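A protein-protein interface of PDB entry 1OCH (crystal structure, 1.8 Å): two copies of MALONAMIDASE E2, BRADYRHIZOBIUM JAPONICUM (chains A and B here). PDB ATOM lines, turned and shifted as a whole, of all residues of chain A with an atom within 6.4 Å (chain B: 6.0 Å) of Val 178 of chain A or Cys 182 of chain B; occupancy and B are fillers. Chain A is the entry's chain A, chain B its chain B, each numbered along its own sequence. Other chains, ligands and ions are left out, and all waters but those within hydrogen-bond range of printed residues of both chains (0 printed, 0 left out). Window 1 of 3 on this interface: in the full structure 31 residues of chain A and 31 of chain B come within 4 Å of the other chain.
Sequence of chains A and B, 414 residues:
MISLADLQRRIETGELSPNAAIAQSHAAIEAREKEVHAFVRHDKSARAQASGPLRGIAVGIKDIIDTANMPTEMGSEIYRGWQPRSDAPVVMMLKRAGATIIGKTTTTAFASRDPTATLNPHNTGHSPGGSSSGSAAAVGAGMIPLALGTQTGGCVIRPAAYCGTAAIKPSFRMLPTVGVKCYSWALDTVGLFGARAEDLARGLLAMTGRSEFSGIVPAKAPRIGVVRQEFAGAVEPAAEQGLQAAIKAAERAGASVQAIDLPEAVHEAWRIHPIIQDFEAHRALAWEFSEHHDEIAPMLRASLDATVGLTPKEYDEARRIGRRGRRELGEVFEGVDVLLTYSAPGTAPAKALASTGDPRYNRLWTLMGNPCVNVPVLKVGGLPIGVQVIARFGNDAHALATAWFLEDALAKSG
SG of Cys 182 of chain B sits at hydrogen-bond distance from N of Ser 184 of chain B, 3.7 Å away.
SG of Cys 182 of chain B is in hydrogen-bond range of N of Trp 185 of chain B, at 3.5 Å.
The side-chain sulfur (SG) of Cys 182 of chain B lies close to the side-chain carboxylate (OD2) of Asp 188 of chain B (3.6 Å).
1 position is printed for both chains.
Of the 3 pairs that touch across the chains among the printed residues, none has its exchanged pair printed and touching as well.
Hydrophobic or aromatic side chains of chain B within 4 Å of the printed part of chain A: Trp 185.
Of the 12 printed residues of chain A, 3 touch a printed residue of chain B.
Along chain A the printed residues that touch a printed residue of chain B span positions 89 to 178.
Among the printed residues, 3 pairs touch across the chains.
Asp 87 of chain A touches none of the printed residues of chain B.
Of the printed residues of chain B, Pro 89 of chain A touches Ala 284 (3.8 Å).
Leu 175 of chain A touches none of the printed residues of chain B.
Of the printed residues of chain B, Pro 176 of chain A touches Trp 185 (3.7 Å).
Of chain B, only Cys 182 comes within 4 Å of Val 178 of chain A.
Cys 182 of chain B touches just one residue of chain A: Val 178 (3.6 Å).
Of the printed residues of chain A, Trp 185 of chain B touches Pro 176.
Printed residues of chain A within 4 Å of Ala 284 of chain B: Pro 89.
The nearest residue of chain B that does not touch Val 178 of chain A is Trp 185 of chain B (4.4 Å).
The nearest printed residue of chain A that does not touch Cys 182 of chain B is Pro 176 of chain A (6.8 Å).
The nearest printed residue of chain A that does not touch Trp 185 of chain B is Val 178 of chain A (4.4 Å).
CG of Pro 89 of chain A touches CA of Ala 284 of chain B, at 3.8 Å.
Pro 176 of chain A touches Trp 185 of chain B.
Cys 182 of chain B touches Val 178 of chain A.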
ATOM      1  N   ILE A  65     -35.091  25.823  -2.486  1.00  0.00           N
ATOM      2  CA  ILE A  65     -34.086  25.057  -3.214  1.00  0.00           C
ATOM      3  C   ILE A  65     -32.794  25.884  -3.246  1.00  0.00           C
ATOM      4  O   ILE A  65     -32.788  27.022  -3.723  1.00  0.00           O
ATOM      5  CB  ILE A  65     -34.567  24.749  -4.653  1.00  0.00           C
ATOM      6  CG1 ILE A  65     -35.867  23.937  -4.600  1.00  0.00           C
ATOM      7  CG2 ILE A  65     -33.499  23.987  -5.408  1.00  0.00           C
ATOM      8  CD1 ILE A  65     -36.518  23.718  -5.951  1.00  0.00           C
ATOM      9  N   ASP A  66     -31.713  25.307  -2.721  1.00  0.00           N
ATOM     10  CA  ASP A  66     -30.410  25.978  -2.635  1.00  0.00           C
ATOM     11  C   ASP A  66     -29.778  26.451  -3.936  1.00  0.00           C
ATOM     12  O   ASP A  66     -29.715  25.708  -4.914  1.00  0.00           O
ATOM     13  CB  ASP A  66     -29.373  25.076  -1.947  1.00  0.00           C
ATOM     14  CG  ASP A  66     -29.607  24.919  -0.459  1.00  0.00           C
ATOM     15  OD1 ASP A  66     -30.462  25.630   0.110  1.00  0.00           O
ATOM     16  OD2 ASP A  66     -28.913  24.075   0.145  1.00  0.00           O
ATOM     17  N   ASP A  87     -25.105  24.831  -5.010  1.00  0.00           N
ATOM     18  CA  ASP A  87     -26.355  24.730  -5.742  1.00  0.00           C
ATOM     19  C   ASP A  87     -26.865  23.335  -5.454  1.00  0.00           C
ATOM     20  O   ASP A  87     -26.080  22.381  -5.418  1.00  0.00           O
ATOM     21  CB  ASP A  87     -26.147  24.844  -7.257  1.00  0.00           C
ATOM     22  CG  ASP A  87     -25.842  26.247  -7.701  1.00  0.00           C
ATOM     23  OD1 ASP A  87     -26.587  27.166  -7.310  1.00  0.00           O
ATOM     24  OD2 ASP A  87     -24.866  26.424  -8.454  1.00  0.00           O
ATOM     25  N   ALA A  88     -28.169  23.213  -5.252  1.00  0.00           N
ATOM     26  CA  ALA A  88     -28.767  21.921  -4.985  1.00  0.00           C
ATOM     27  C   ALA A  88     -28.561  21.037  -6.206  1.00  0.00           C
ATOM     28  O   ALA A  88     -28.448  21.527  -7.327  1.00  0.00           O
ATOM     29  CB  ALA A  88     -30.255  22.079  -4.693  1.00  0.00           C
ATOM     30  N   PRO A  89     -28.486  19.720  -6.001  1.00  0.00           N
ATOM     31  CA  PRO A  89     -28.296  18.831  -7.144  1.00  0.00           C
ATOM     32  C   PRO A  89     -29.277  19.053  -8.306  1.00  0.00           C
ATOM     33  O   PRO A  89     -28.879  18.963  -9.467  1.00  0.00           O
ATOM     34  CB  PRO A  89     -28.412  17.455  -6.509  1.00  0.00           C
ATOM     35  CG  PRO A  89     -27.675  17.676  -5.202  1.00  0.00           C
ATOM     36  CD  PRO A  89     -28.268  18.998  -4.733  1.00  0.00           C
ATOM     37  N   VAL A  90     -30.545  19.344  -8.020  1.00  0.00           N
ATOM     38  CA  VAL A  90     -31.493  19.561  -9.116  1.00  0.00           C
ATOM     39  C   VAL A  90     -31.172  20.840  -9.881  1.00  0.00           C
ATOM     40  O   VAL A  90     -31.451  20.936 -11.075  1.00  0.00           O
ATOM     41  CB  VAL A  90     -32.971  19.608  -8.640  1.00  0.00           C
ATOM     42  CG1 VAL A  90     -33.415  18.225  -8.188  1.00  0.00           C
ATOM     43  CG2 VAL A  90     -33.136  20.619  -7.529  1.00  0.00           C
ATOM     44  N   LEU A 175     -35.998  12.576  -8.515  1.00  0.00           N
ATOM     45  CA  LEU A 175     -35.135  13.757  -8.481  1.00  0.00           C
ATOM     46  C   LEU A 175     -34.690  13.922  -7.030  1.00  0.00           C
ATOM     47  O   LEU A 175     -35.507  13.873  -6.113  1.00  0.00           O
ATOM     48  CB  LEU A 175     -35.895  15.011  -8.934  1.00  0.00           C
ATOM     49  CG  LEU A 175     -36.374  15.064 -10.390  1.00  0.00           C
ATOM     50  CD1 LEU A 175     -37.154  16.348 -10.621  1.00  0.00           C
ATOM     51  CD2 LEU A 175     -35.177  14.987 -11.339  1.00  0.00           C
ATOM     52  N   PRO A 176     -33.387  14.119  -6.801  1.00  0.00           N
ATOM     53  CA  PRO A 176     -32.917  14.274  -5.422  1.00  0.00           C
ATOM     54  C   PRO A 176     -33.464  15.504  -4.705  1.00  0.00           C
ATOM     55  O   PRO A 176     -33.660  16.557  -5.313  1.00  0.00           O
ATOM     56  CB  PRO A 176     -31.400  14.329  -5.583  1.00  0.00           C
ATOM     57  CG  PRO A 176     -31.241  15.016  -6.914  1.00  0.00           C
ATOM     58  CD  PRO A 176     -32.291  14.337  -7.765  1.00  0.00           C
ATOM     59  N   THR A 177     -33.712  15.361  -3.405  1.00  0.00           N
ATOM     60  CA  THR A 177     -34.195  16.472  -2.605  1.00  0.00           C
ATOM     61  C   THR A 177     -33.037  17.038  -1.790  1.00  0.00           C
ATOM     62  O   THR A 177     -33.240  17.800  -0.847  1.00  0.00           O
ATOM     63  CB  THR A 177     -35.337  16.051  -1.661  1.00  0.00           C
ATOM     64  OG1 THR A 177     -34.953  14.881  -0.934  1.00  0.00           O
ATOM     65  CG2 THR A 177     -36.608  15.773  -2.462  1.00  0.00           C
ATOM     66  N   VAL A 178     -31.817  16.640  -2.151  1.00  0.00           N
ATOM     67  CA  VAL A 178     -30.624  17.155  -1.491  1.00  0.00           C
ATOM     68  C   VAL A 178     -30.636  18.658  -1.786  1.00  0.00           C
ATOM     69  O   VAL A 178     -30.888  19.066  -2.919  1.00  0.00           O
ATOM     70  CB  VAL A 178     -29.333  16.544  -2.096  1.00  0.00           C
ATOM     71  CG1 VAL A 178     -28.096  17.289  -1.572  1.00  0.00           C
ATOM     72  CG2 VAL A 178     -29.241  15.072  -1.741  1.00  0.00           C
ATOM     73  N   GLY A 179     -30.383  19.475  -0.770  1.00  0.00           N
ATOM     74  CA  GLY A 179     -30.380  20.911  -0.973  1.00  0.00           C
ATOM     75  C   GLY A 179     -31.774  21.500  -1.111  1.00  0.00           C
ATOM     76  O   GLY A 179     -31.931  22.614  -1.610  1.00  0.00           O
ATOM     77  N   VAL A 180     -32.784  20.751  -0.677  1.00  0.00           N
ATOM     78  CA  VAL A 180     -34.172  21.200  -0.731  1.00  0.00           C
ATOM     79  C   VAL A 180     -34.704  21.207   0.707  1.00  0.00           C
ATOM     80  O   VAL A 180     -34.782  20.159   1.343  1.00  0.00           O
ATOM     81  CB  VAL A 180     -35.031  20.242  -1.587  1.00  0.00           C
ATOM     82  CG1 VAL A 180     -36.477  20.720  -1.624  1.00  0.00           C
ATOM     83  CG2 VAL A 180     -34.462  20.161  -3.003  1.00  0.00           C
ATOM     84  N   PHE B 110     -16.127  14.638   2.458  1.00  0.00           N
ATOM     85  CA  PHE B 110     -17.426  14.196   1.975  1.00  0.00           C
ATOM     86  C   PHE B 110     -17.720  12.723   2.308  1.00  0.00           C
ATOM     87  O   PHE B 110     -18.429  12.034   1.571  1.00  0.00           O
ATOM     88  CB  PHE B 110     -17.532  14.440   0.466  1.00  0.00           C
ATOM     89  CG  PHE B 110     -17.275  15.866   0.073  1.00  0.00           C
ATOM     90  CD1 PHE B 110     -16.073  16.231  -0.523  1.00  0.00           C
ATOM     91  CD2 PHE B 110     -18.219  16.856   0.345  1.00  0.00           C
ATOM     92  CE1 PHE B 110     -15.811  17.564  -0.841  1.00  0.00           C
ATOM     93  CE2 PHE B 110     -17.965  18.188   0.032  1.00  0.00           C
ATOM     94  CZ  PHE B 110     -16.757  18.543  -0.563  1.00  0.00           C
ATOM     95  N   VAL B 180     -27.584  16.363   6.753  1.00  0.00           N
ATOM     96  CA  VAL B 180     -26.454  15.444   6.703  1.00  0.00           C
ATOM     97  C   VAL B 180     -25.956  15.464   5.264  1.00  0.00           C
ATOM     98  O   VAL B 180     -26.682  15.078   4.352  1.00  0.00           O
ATOM     99  CB  VAL B 180     -26.868  13.999   7.085  1.00  0.00           C
ATOM    100  CG1 VAL B 180     -25.655  13.075   7.032  1.00  0.00           C
ATOM    101  CG2 VAL B 180     -27.471  13.981   8.481  1.00  0.00           C
ATOM    102  N   LYS B 181     -24.726  15.934   5.065  1.00  0.00           N
ATOM    103  CA  LYS B 181     -24.140  16.025   3.733  1.00  0.00           C
ATOM    104  C   LYS B 181     -24.317  14.710   3.005  1.00  0.00           C
ATOM    105  O   LYS B 181     -23.776  13.683   3.411  1.00  0.00           O
ATOM    106  CB  LYS B 181     -22.657  16.386   3.828  1.00  0.00           C
ATOM    107  CG  LYS B 181     -21.979  16.643   2.488  1.00  0.00           C
ATOM    108  CD  LYS B 181     -22.696  17.714   1.684  1.00  0.00           C
ATOM    109  CE  LYS B 181     -21.866  18.132   0.471  1.00  0.00           C
ATOM    110  NZ  LYS B 181     -22.689  18.873  -0.518  1.00  0.00           N
ATOM    111  N   CYS B 182     -25.068  14.753   1.912  1.00  0.00           N
ATOM    112  CA  CYS B 182     -25.359  13.561   1.152  1.00  0.00           C
ATOM    113  C   CYS B 182     -24.291  13.056   0.193  1.00  0.00           C
ATOM    114  O   CYS B 182     -23.650  13.833  -0.522  1.00  0.00           O
ATOM    115  CB  CYS B 182     -26.662  13.761   0.377  1.00  0.00           C
ATOM    116  SG  CYS B 182     -27.175  12.314  -0.590  1.00  0.00           S
ATOM    117  N   TYR B 183     -24.107  11.736   0.193  1.00  0.00           N
ATOM    118  CA  TYR B 183     -23.180  11.086  -0.716  1.00  0.00           C
ATOM    119  C   TYR B 183     -24.052  10.202  -1.617  1.00  0.00           C
ATOM    120  O   TYR B 183     -23.966  10.272  -2.840  1.00  0.00           O
ATOM    121  CB  TYR B 183     -22.153  10.240   0.037  1.00  0.00           C
ATOM    122  CG  TYR B 183     -21.062   9.711  -0.871  1.00  0.00           C
ATOM    123  CD1 TYR B 183     -21.256   8.560  -1.634  1.00  0.00           C
ATOM    124  CD2 TYR B 183     -19.845  10.379  -0.990  1.00  0.00           C
ATOM    125  CE1 TYR B 183     -20.264   8.087  -2.488  1.00  0.00           C
ATOM    126  CE2 TYR B 183     -18.850   9.914  -1.840  1.00  0.00           C
ATOM    127  CZ  TYR B 183     -19.065   8.765  -2.586  1.00  0.00           C
ATOM    128  OH  TYR B 183     -18.069   8.291  -3.413  1.00  0.00           O
ATOM    129  N   SER B 184     -24.889   9.376  -0.989  1.00  0.00           N
ATOM    130  CA  SER B 184     -25.834   8.501  -1.687  1.00  0.00           C
ATOM    131  C   SER B 184     -27.114   8.485  -0.840  1.00  0.00           C
ATOM    132  O   SER B 184     -27.127   7.943   0.265  1.00  0.00           O
ATOM    133  CB  SER B 184     -25.286   7.076  -1.818  1.00  0.00           C
ATOM    134  OG  SER B 184     -26.265   6.219  -2.390  1.00  0.00           O
ATOM    135  N   TRP B 185     -28.183   9.088  -1.353  1.00  0.00           N
ATOM    136  CA  TRP B 185     -29.428   9.150  -0.603  1.00  0.00           C
ATOM    137  C   TRP B 185     -30.111   7.805  -0.442  1.00  0.00           C
ATOM    138  O   TRP B 185     -30.962   7.628   0.426  1.00  0.00           O
ATOM    139  CB  TRP B 185     -30.384  10.178  -1.233  1.00  0.00           C
ATOM    140  CG  TRP B 185     -30.795   9.918  -2.656  1.00  0.00           C
ATOM    141  CD1 TRP B 185     -31.841   9.148  -3.082  1.00  0.00           C
ATOM    142  CD2 TRP B 185     -30.201  10.475  -3.839  1.00  0.00           C
ATOM    143  NE1 TRP B 185     -31.941   9.198  -4.454  1.00  0.00           N
ATOM    144  CE2 TRP B 185     -30.945  10.004  -4.944  1.00  0.00           C
ATOM    145  CE3 TRP B 185     -29.111  11.328  -4.071  1.00  0.00           C
ATOM    146  CZ2 TRP B 185     -30.636  10.360  -6.266  1.00  0.00           C
ATOM    147  CZ3 TRP B 185     -28.804  11.682  -5.385  1.00  0.00           C
ATOM    148  CH2 TRP B 185     -29.565  11.197  -6.465  1.00  0.00           C
ATOM    149  N   ASP B 188     -26.980   6.504   2.578  1.00  0.00           N
ATOM    150  CA  ASP B 188     -26.688   7.290   3.779  1.00  0.00           C
ATOM    151  C   ASP B 188     -27.606   6.980   4.964  1.00  0.00           C
ATOM    152  O   ASP B 188     -28.828   7.093   4.866  1.00  0.00           O
ATOM    153  CB  ASP B 188     -26.758   8.790   3.473  1.00  0.00           C
ATOM    154  CG  ASP B 188     -25.691   9.245   2.487  1.00  0.00           C
ATOM    155  OD1 ASP B 188     -24.847   8.415   2.077  1.00  0.00           O
ATOM    156  OD2 ASP B 188     -25.702  10.444   2.124  1.00  0.00           O
ATOM    157  N   ALA B 284     -25.369  14.017  -6.181  1.00  0.00           N
ATOM    158  CA  ALA B 284     -25.313  14.657  -4.862  1.00  0.00           C
ATOM    159  C   ALA B 284     -24.140  15.615  -4.673  1.00  0.00           C
ATOM    160  O   ALA B 284     -24.211  16.541  -3.863  1.00  0.00           O
ATOM    161  CB  ALA B 284     -25.287  13.593  -3.770  1.00  0.00           C
ATOM    162  N   LEU B 285     -23.060  15.382  -5.406  1.00  0.00           N
ATOM    163  CA  LEU B 285     -21.879  16.225  -5.308  1.00  0.00           C
ATOM    164  C   LEU B 285     -21.642  16.954  -6.629  1.00  0.00           C
ATOM    165  O   LEU B 285     -20.509  17.305  -6.955  1.00  0.00           O
ATOM    166  CB  LEU B 285     -20.654  15.370  -4.957  1.00  0.00           C
ATOM    167  CG  LEU B 285     -20.681  14.614  -3.624  1.00  0.00           C
ATOM    168  CD1 LEU B 285     -19.502  13.640  -3.549  1.00  0.00           C
ATOM    169  CD2 LEU B 285     -20.637  15.609  -2.476  1.00  0.00           C
